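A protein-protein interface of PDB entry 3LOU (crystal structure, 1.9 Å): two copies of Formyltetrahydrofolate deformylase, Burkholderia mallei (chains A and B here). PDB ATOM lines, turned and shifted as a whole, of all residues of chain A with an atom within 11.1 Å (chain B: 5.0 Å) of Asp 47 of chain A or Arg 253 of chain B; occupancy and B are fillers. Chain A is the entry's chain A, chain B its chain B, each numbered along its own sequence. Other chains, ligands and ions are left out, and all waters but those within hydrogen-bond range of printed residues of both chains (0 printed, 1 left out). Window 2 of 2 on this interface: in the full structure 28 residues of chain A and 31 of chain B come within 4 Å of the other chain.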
ATOM      1  N   CYS A  17      -1.215  -4.436  -5.925  1.00  0.00           N
ATOM      2  CA  CYS A  17      -1.475  -3.583  -7.074  1.00  0.00           C
ATOM      3  C   CYS A  17      -0.751  -4.115  -8.305  1.00  0.00           C
ATOM      4  O   CYS A  17       0.067  -5.030  -8.187  1.00  0.00           O
ATOM      5  CB  CYS A  17      -1.015  -2.163  -6.755  1.00  0.00           C
ATOM      6  SG  CYS A  17       0.781  -2.018  -6.454  1.00  0.00           S
ATOM      7  N   PRO A  18      -1.063  -3.564  -9.498  1.00  0.00           N
ATOM      8  CA  PRO A  18      -0.361  -4.014 -10.698  1.00  0.00           C
ATOM      9  C   PRO A  18       1.088  -3.611 -10.620  1.00  0.00           C
ATOM     10  O   PRO A  18       1.397  -2.553 -10.080  1.00  0.00           O
ATOM     11  CB  PRO A  18      -1.060  -3.256 -11.825  1.00  0.00           C
ATOM     12  CG  PRO A  18      -2.401  -2.956 -11.294  1.00  0.00           C
ATOM     13  CD  PRO A  18      -2.180  -2.677  -9.834  1.00  0.00           C
ATOM     14  N   SER A  19       1.965  -4.451 -11.155  1.00  0.00           N
ATOM     15  CA  SER A  19       3.390  -4.169 -11.186  1.00  0.00           C
ATOM     16  C   SER A  19       3.645  -2.845 -11.874  1.00  0.00           C
ATOM     17  O   SER A  19       3.019  -2.520 -12.902  1.00  0.00           O
ATOM     18  CB  SER A  19       4.161  -5.317 -11.882  1.00  0.00           C
ATOM     19  OG  SER A  19       3.972  -6.557 -11.197  1.00  0.00           O
ATOM     20  N   ALA A  20       4.547  -2.072 -11.278  1.00  0.00           N
ATOM     21  CA  ALA A  20       4.944  -0.748 -11.763  1.00  0.00           C
ATOM     22  C   ALA A  20       6.025  -0.241 -10.820  1.00  0.00           C
ATOM     23  O   ALA A  20       6.231  -0.805  -9.741  1.00  0.00           O
ATOM     24  CB  ALA A  20       3.753   0.220 -11.782  1.00  0.00           C
ATOM     25  N   VAL A  43       8.202  -7.112   0.712  1.00  0.00           N
ATOM     26  CA  VAL A  43       7.768  -6.764  -0.597  1.00  0.00           C
ATOM     27  C   VAL A  43       7.952  -7.947  -1.505  1.00  0.00           C
ATOM     28  O   VAL A  43       8.974  -8.636  -1.414  1.00  0.00           O
ATOM     29  CB  VAL A  43       8.625  -5.587  -1.102  1.00  0.00           C
ATOM     30  CG1 VAL A  43       8.284  -5.190  -2.514  1.00  0.00           C
ATOM     31  CG2 VAL A  43       8.444  -4.390  -0.159  1.00  0.00           C
ATOM     32  N   PHE A  44       7.013  -8.134  -2.430  1.00  0.00           N
ATOM     33  CA  PHE A  44       7.093  -9.205  -3.407  1.00  0.00           C
ATOM     34  C   PHE A  44       6.454  -8.803  -4.698  1.00  0.00           C
ATOM     35  O   PHE A  44       5.297  -8.372  -4.698  1.00  0.00           O
ATOM     36  CB  PHE A  44       6.377 -10.431  -2.894  1.00  0.00           C
ATOM     37  CG  PHE A  44       6.342 -11.562  -3.887  1.00  0.00           C
ATOM     38  CD1 PHE A  44       7.537 -12.134  -4.356  1.00  0.00           C
ATOM     39  CD2 PHE A  44       5.130 -12.077  -4.334  1.00  0.00           C
ATOM     40  CE1 PHE A  44       7.515 -13.165  -5.274  1.00  0.00           C
ATOM     41  CE2 PHE A  44       5.114 -13.158  -5.271  1.00  0.00           C
ATOM     42  CZ  PHE A  44       6.309 -13.660  -5.756  1.00  0.00           C
ATOM     43  N   ASP A  45       7.217  -8.889  -5.784  1.00  0.00           N
ATOM     44  CA  ASP A  45       6.695  -8.661  -7.096  1.00  0.00           C
ATOM     45  C   ASP A  45       6.605  -9.987  -7.823  1.00  0.00           C
ATOM     46  O   ASP A  45       7.583 -10.718  -7.924  1.00  0.00           O
ATOM     47  CB  ASP A  45       7.557  -7.684  -7.926  1.00  0.00           C
ATOM     48  CG  ASP A  45       6.849  -7.275  -9.264  1.00  0.00           C
ATOM     49  OD1 ASP A  45       5.806  -6.573  -9.253  1.00  0.00           O
ATOM     50  OD2 ASP A  45       7.303  -7.700 -10.318  1.00  0.00           O
ATOM     51  N   ASP A  46       5.419 -10.301  -8.325  1.00  0.00           N
ATOM     52  CA  ASP A  46       5.219 -11.515  -9.092  1.00  0.00           C
ATOM     53  C   ASP A  46       5.192 -11.124 -10.542  1.00  0.00           C
ATOM     54  O   ASP A  46       4.189 -10.628 -11.047  1.00  0.00           O
ATOM     55  CB  ASP A  46       3.928 -12.168  -8.682  1.00  0.00           C
ATOM     56  CG  ASP A  46       3.718 -13.475  -9.353  1.00  0.00           C
ATOM     57  OD1 ASP A  46       4.183 -13.646 -10.508  1.00  0.00           O
ATOM     58  OD2 ASP A  46       3.061 -14.328  -8.737  1.00  0.00           O
ATOM     59  N   ASP A  47       6.310 -11.333 -11.216  1.00  0.00           N
ATOM     60  CA  ASP A  47       6.436 -10.921 -12.596  1.00  0.00           C
ATOM     61  C   ASP A  47       5.633 -11.813 -13.524  1.00  0.00           C
ATOM     62  O   ASP A  47       5.414 -11.448 -14.648  1.00  0.00           O
ATOM     63  CB  ASP A  47       7.904 -10.849 -13.033  1.00  0.00           C
ATOM     64  CG  ASP A  47       8.629 -12.155 -12.863  1.00  0.00           C
ATOM     65  OD1 ASP A  47       8.726 -12.638 -11.705  1.00  0.00           O
ATOM     66  OD2 ASP A  47       9.124 -12.674 -13.880  1.00  0.00           O
ATOM     67  N   LEU A  48       5.143 -12.960 -13.048  1.00  0.00           N
ATOM     68  CA  LEU A  48       4.297 -13.784 -13.922  1.00  0.00           C
ATOM     69  C   LEU A  48       2.822 -13.299 -13.922  1.00  0.00           C
ATOM     70  O   LEU A  48       2.182 -13.238 -14.975  1.00  0.00           O
ATOM     71  CB  LEU A  48       4.464 -15.283 -13.580  1.00  0.00           C
ATOM     72  CG  LEU A  48       5.945 -15.719 -13.847  1.00  0.00           C
ATOM     73  CD1 LEU A  48       6.209 -17.207 -13.538  1.00  0.00           C
ATOM     74  CD2 LEU A  48       6.388 -15.401 -15.297  1.00  0.00           C
ATOM     75  N   SER A  49       2.300 -12.918 -12.760  1.00  0.00           N
ATOM     76  CA  SER A  49       0.959 -12.398 -12.666  1.00  0.00           C
ATOM     77  C   SER A  49       0.980 -10.863 -12.761  1.00  0.00           C
ATOM     78  O   SER A  49      -0.070 -10.232 -12.822  1.00  0.00           O
ATOM     79  CB  SER A  49       0.306 -12.824 -11.353  1.00  0.00           C
ATOM     80  OG  SER A  49       1.000 -12.264 -10.239  1.00  0.00           O
ATOM     81  N   ALA A  50       2.184 -10.267 -12.781  1.00  0.00           N
ATOM     82  CA  ALA A  50       2.317  -8.792 -12.876  1.00  0.00           C
ATOM     83  C   ALA A  50       1.588  -8.119 -11.713  1.00  0.00           C
ATOM     84  O   ALA A  50       0.885  -7.123 -11.882  1.00  0.00           O
ATOM     85  CB  ALA A  50       1.793  -8.296 -14.225  1.00  0.00           C
ATOM     86  N   ARG A  51       1.795  -8.664 -10.523  1.00  0.00           N
ATOM     87  CA  ARG A  51       1.180  -8.160  -9.318  1.00  0.00           C
ATOM     88  C   ARG A  51       2.256  -7.937  -8.253  1.00  0.00           C
ATOM     89  O   ARG A  51       3.199  -8.741  -8.104  1.00  0.00           O
ATOM     90  CB  ARG A  51       0.168  -9.163  -8.815  1.00  0.00           C
ATOM     91  CG  ARG A  51      -0.769  -8.651  -7.852  1.00  0.00           C
ATOM     92  CD  ARG A  51      -2.024  -8.081  -8.506  1.00  0.00           C
ATOM     93  NE  ARG A  51      -2.885  -7.544  -7.461  1.00  0.00           N
ATOM     94  CZ  ARG A  51      -3.770  -6.576  -7.634  1.00  0.00           C
ATOM     95  NH1 ARG A  51      -3.925  -6.029  -8.835  1.00  0.00           N
ATOM     96  NH2 ARG A  51      -4.491  -6.148  -6.598  1.00  0.00           N
ATOM     97  N   PHE A  52       2.076  -6.871  -7.503  1.00  0.00           N
ATOM     98  CA  PHE A  52       3.017  -6.426  -6.504  1.00  0.00           C
ATOM     99  C   PHE A  52       2.345  -6.415  -5.141  1.00  0.00           C
ATOM    100  O   PHE A  52       1.180  -6.028  -5.017  1.00  0.00           O
ATOM    101  CB  PHE A  52       3.508  -5.026  -6.896  1.00  0.00           C
ATOM    102  CG  PHE A  52       4.560  -4.488  -6.010  1.00  0.00           C
ATOM    103  CD1 PHE A  52       5.845  -5.007  -6.049  1.00  0.00           C
ATOM    104  CD2 PHE A  52       4.289  -3.405  -5.154  1.00  0.00           C
ATOM    105  CE1 PHE A  52       6.835  -4.498  -5.215  1.00  0.00           C
ATOM    106  CE2 PHE A  52       5.267  -2.881  -4.362  1.00  0.00           C
ATOM    107  CZ  PHE A  52       6.545  -3.429  -4.373  1.00  0.00           C
ATOM    108  N   PHE A  53       3.093  -6.806  -4.110  1.00  0.00           N
ATOM    109  CA  PHE A  53       2.569  -6.949  -2.767  1.00  0.00           C
ATOM    110  C   PHE A  53       3.475  -6.317  -1.712  1.00  0.00           C
ATOM    111  O   PHE A  53       4.682  -6.523  -1.723  1.00  0.00           O
ATOM    112  CB  PHE A  53       2.443  -8.440  -2.422  1.00  0.00           C
ATOM    113  CG  PHE A  53       1.607  -9.201  -3.394  1.00  0.00           C
ATOM    114  CD1 PHE A  53       2.141  -9.660  -4.561  1.00  0.00           C
ATOM    115  CD2 PHE A  53       0.261  -9.380  -3.168  1.00  0.00           C
ATOM    116  CE1 PHE A  53       1.347 -10.327  -5.494  1.00  0.00           C
ATOM    117  CE2 PHE A  53      -0.509 -10.026  -4.086  1.00  0.00           C
ATOM    118  CZ  PHE A  53       0.035 -10.506  -5.239  1.00  0.00           C
ATOM    119  N   ASN A 284      -3.560 -13.718  -5.015  1.00  0.00           N
ATOM    120  CA  ASN A 284      -2.786 -13.498  -6.232  1.00  0.00           C
ATOM    121  C   ASN A 284      -3.407 -14.367  -7.342  1.00  0.00           C
ATOM    122  O   ASN A 284      -2.827 -15.363  -7.795  1.00  0.00           O
ATOM    123  CB  ASN A 284      -1.326 -13.864  -5.973  1.00  0.00           C
ATOM    124  CG  ASN A 284      -0.424 -13.558  -7.119  1.00  0.00           C
ATOM    125  OD1 ASN A 284      -0.777 -12.806  -8.040  1.00  0.00           O
ATOM    126  ND2 ASN A 284       0.789 -14.150  -7.090  1.00  0.00           N
ATOM    127  N   ARG A 287      -3.809 -18.233  -6.857  1.00  0.00           N
ATOM    128  CA  ARG A 287      -2.906 -18.615  -5.784  1.00  0.00           C
ATOM    129  C   ARG A 287      -2.814 -17.527  -4.706  1.00  0.00           C
ATOM    130  O   ARG A 287      -3.571 -16.556  -4.735  1.00  0.00           O
ATOM    131  CB  ARG A 287      -1.519 -18.983  -6.346  1.00  0.00           C
ATOM    132  CG  ARG A 287      -0.820 -17.939  -7.145  1.00  0.00           C
ATOM    133  CD  ARG A 287       0.484 -18.503  -7.767  1.00  0.00           C
ATOM    134  NE  ARG A 287       1.206 -17.473  -8.495  1.00  0.00           N
ATOM    135  CZ  ARG A 287       0.892 -17.081  -9.719  1.00  0.00           C
ATOM    136  NH1 ARG A 287      -0.116 -17.631 -10.347  1.00  0.00           N
ATOM    137  NH2 ARG A 287       1.584 -16.136 -10.315  1.00  0.00           N
ATOM    138  N   VAL A 289      -0.078 -15.311  -1.859  1.00  0.00           N
ATOM    139  CA  VAL A 289       1.247 -14.879  -1.374  1.00  0.00           C
ATOM    140  C   VAL A 289       1.066 -14.910   0.145  1.00  0.00           C
ATOM    141  O   VAL A 289       0.108 -14.295   0.680  1.00  0.00           O
ATOM    142  CB  VAL A 289       1.594 -13.473  -1.858  1.00  0.00           C
ATOM    143  CG1 VAL A 289       2.847 -12.890  -1.116  1.00  0.00           C
ATOM    144  CG2 VAL A 289       1.811 -13.459  -3.408  1.00  0.00           C
ATOM    145  N   HIS B 217       3.426 -24.076  -9.978  1.00  0.00           N
ATOM    146  CA  HIS B 217       3.648 -22.679  -9.705  1.00  0.00           C
ATOM    147  C   HIS B 217       2.331 -21.907  -9.846  1.00  0.00           C
ATOM    148  O   HIS B 217       2.012 -21.058  -9.007  1.00  0.00           O
ATOM    149  CB  HIS B 217       4.683 -22.074 -10.659  1.00  0.00           C
ATOM    150  CG  HIS B 217       4.815 -20.601 -10.515  1.00  0.00           C
ATOM    151  ND1 HIS B 217       4.062 -19.713 -11.247  1.00  0.00           N
ATOM    152  CD2 HIS B 217       5.577 -19.856  -9.681  1.00  0.00           C
ATOM    153  CE1 HIS B 217       4.362 -18.480 -10.875  1.00  0.00           C
ATOM    154  NE2 HIS B 217       5.285 -18.541  -9.930  1.00  0.00           N
ATOM    155  N   SER B 251       7.549 -17.401  -3.777  1.00  0.00           N
ATOM    156  CA  SER B 251       8.758 -16.771  -4.387  1.00  0.00           C
ATOM    157  C   SER B 251       9.524 -17.703  -5.321  1.00  0.00           C
ATOM    158  O   SER B 251      10.457 -17.278  -6.041  1.00  0.00           O
ATOM    159  CB  SER B 251       9.711 -16.266  -3.281  1.00  0.00           C
ATOM    160  OG  SER B 251      10.339 -17.342  -2.583  1.00  0.00           O
ATOM    161  N   TYR B 252       9.134 -18.964  -5.333  1.00  0.00           N
ATOM    162  CA  TYR B 252       9.779 -19.942  -6.166  1.00  0.00           C
ATOM    163  C   TYR B 252       9.196 -19.913  -7.554  1.00  0.00           C
ATOM    164  O   TYR B 252       8.042 -20.290  -7.760  1.00  0.00           O
ATOM    165  CB  TYR B 252       9.595 -21.356  -5.586  1.00  0.00           C
ATOM    166  CG  TYR B 252      10.449 -21.673  -4.363  1.00  0.00           C
ATOM    167  CD1 TYR B 252      10.290 -20.970  -3.178  1.00  0.00           C
ATOM    168  CD2 TYR B 252      11.397 -22.695  -4.394  1.00  0.00           C
ATOM    169  CE1 TYR B 252      11.047 -21.259  -2.073  1.00  0.00           C
ATOM    170  CE2 TYR B 252      12.160 -22.983  -3.314  1.00  0.00           C
ATOM    171  CZ  TYR B 252      11.985 -22.282  -2.142  1.00  0.00           C
ATOM    172  OH  TYR B 252      12.745 -22.587  -1.039  1.00  0.00           O
ATOM    173  N   ARG B 253      10.017 -19.499  -8.526  1.00  0.00           N
ATOM    174  CA  ARG B 253       9.631 -19.544  -9.897  1.00  0.00           C
ATOM    175  C   ARG B 253       9.552 -21.004 -10.336  1.00  0.00           C
ATOM    176  O   ARG B 253      10.068 -21.879  -9.640  1.00  0.00           O
ATOM    177  CB  ARG B 253      10.659 -18.777 -10.741  1.00  0.00           C
ATOM    178  CG  ARG B 253      10.941 -17.325 -10.202  1.00  0.00           C
ATOM    179  CD  ARG B 253      12.029 -16.639 -11.029  1.00  0.00           C
ATOM    180  NE  ARG B 253      11.701 -16.768 -12.436  1.00  0.00           N
ATOM    181  CZ  ARG B 253      10.808 -16.003 -13.056  1.00  0.00           C
ATOM    182  NH1 ARG B 253      10.174 -15.045 -12.389  1.00  0.00           N
ATOM    183  NH2 ARG B 253      10.553 -16.188 -14.350  1.00  0.00           N
ATOM    184  N   PRO B 254       8.915 -21.281 -11.484  1.00  0.00           N
ATOM    185  CA  PRO B 254       8.798 -22.663 -11.948  1.00  0.00           C
ATOM    186  C   PRO B 254      10.123 -23.407 -12.044  1.00  0.00           C
ATOM    187  O   PRO B 254      10.192 -24.580 -11.643  1.00  0.00           O
ATOM    188  CB  PRO B 254       8.141 -22.518 -13.323  1.00  0.00           C
ATOM    189  CG  PRO B 254       7.370 -21.261 -13.213  1.00  0.00           C
ATOM    190  CD  PRO B 254       8.276 -20.352 -12.444  1.00  0.00           C
ATOM    191  N   GLU B 255      11.177 -22.733 -12.482  1.00  0.00           N
ATOM    192  CA  GLU B 255      12.498 -23.377 -12.573  1.00  0.00           C
ATOM    193  C   GLU B 255      13.091 -23.686 -11.191  1.00  0.00           C
ATOM    194  O   GLU B 255      13.859 -24.658 -11.037  1.00  0.00           O
ATOM    195  CB  GLU B 255      13.484 -22.560 -13.437  1.00  0.00           C
ATOM    196  CG  GLU B 255      13.720 -21.139 -12.996  1.00  0.00           C
ATOM    197  CD  GLU B 255      12.717 -20.121 -13.609  1.00  0.00           C
ATOM    198  OE1 GLU B 255      11.506 -20.465 -13.876  1.00  0.00           O
ATOM    199  OE2 GLU B 255      13.158 -18.965 -13.798  1.00  0.00           O
ATOM    200  N   GLN B 256      12.731 -22.893 -10.177  1.00  0.00           N
ATOM    201  CA  GLN B 256      13.181 -23.168  -8.832  1.00  0.00           C
ATOM    202  C   GLN B 256      12.391 -24.317  -8.213  1.00  0.00           C
ATOM    203  O   GLN B 256      12.943 -25.108  -7.441  1.00  0.00           O
ATOM    204  CB  GLN B 256      13.094 -21.910  -7.962  1.00  0.00           C
ATOM    205  CG  GLN B 256      14.016 -20.805  -8.460  1.00  0.00           C
ATOM    206  CD  GLN B 256      13.824 -19.478  -7.723  1.00  0.00           C
ATOM    207  OE1 GLN B 256      12.751 -18.868  -7.790  1.00  0.00           O
ATOM    208  NE2 GLN B 256      14.894 -18.999  -7.062  1.00  0.00           N
ATOM    209  N   LEU B 257      11.106 -24.431  -8.541  1.00  0.00           N
ATOM    210  CA  LEU B 257      10.330 -25.590  -8.096  1.00  0.00           C
ATOM    211  C   LEU B 257      10.914 -26.876  -8.689  1.00  0.00           C
ATOM    212  O   LEU B 257      10.996 -27.897  -8.016  1.00  0.00           O
ATOM    213  CB  LEU B 257       8.860 -25.453  -8.507  1.00  0.00           C
ATOM    214  CG  LEU B 257       8.098 -24.309  -7.819  1.00  0.00           C
ATOM    215  CD1 LEU B 257       6.694 -24.225  -8.369  1.00  0.00           C
ATOM    216  CD2 LEU B 257       8.059 -24.488  -6.289  1.00  0.00           C
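OD1 of Asp 47 of chain A lies within salt-bridge range of NH1 of Arg 253 of chain B (2.9 Å).
The side-chain carboxylate of Asp 46 of chain A is in hydrogen-bond range of the backbone NH of Leu 48 of chain A. OD2 of Asp 46 of chain A is in salt-bridge range of NH2 of Arg 287 of chain A (2.8 Å). The guanidinium group of Arg 253 of chain B is in salt-bridge range of the side-chain carboxylate of Glu 255 of chain B (3.0 Å). OE1 of Gln 256 of chain B lies close to O of Ser 251 of chain B. The backbone NH of Arg 253 of chain B lies within hydrogen-bond range of the side-chain amide oxygen of Gln 256 of chain B, 2.9 Å away. The backbone NH of Phe 53 of chain A is in hydrogen-bond range of the backbone carbonyl oxygen of Phe 44 of chain A, at 2.8 Å.
Among the printed residues, pairs that only touch across the chains: Arg 287 of chain A with His 217 of chain B (3.2 Å), Leu 48 of chain A with His 217 of chain B (3.5 Å), Phe 44 of chain A with Ser 251 of chain B (3.9 Å) and Leu 48 of chain A with Pro 254 of chain B (3.9 Å).
Of the printed residues of chain B, Phe 44 of chain A touches Ser 251. Asp 47 of chain A touches just one residue of chain B: Arg 253. Printed residues of chain B within 4 Å of Leu 48 of chain A: His 217 (3.5 Å) and Pro 254 (3.9 Å). Printed residues of chain B within 4 Å of Arg 287 of chain A: His 217. Of chain A, only Phe 44 (3.9 Å) comes within 4 Å of Ser 251 of chain B. Of chain A, only Asp 47 (2.9 Å) comes within 4 Å of Arg 253 of chain B. Of the printed residues of chain A, Pro 254 of chain B touches Leu 48 (3.9 Å). No residue of chain A comes within 4 Å of Gln 256 of chain B. No residue of chain A comes within 4 Å of Leu 257 of chain B. The nearest printed residue of chain B that does not touch Asp 47 of chain A is His 217 of chain B (7.1 Å). The nearest printed residue of chain B that does not touch Leu 48 of chain A is Arg 253 of chain B (4.3 Å).
Of the 18 printed residues of chain A, 4 touch a printed residue of chain B. Hydrophobic or aromatic side chains of chain A within 4 Å of the printed part of chain B: Phe 44 and Leu 48.
No position is printed for both chains.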
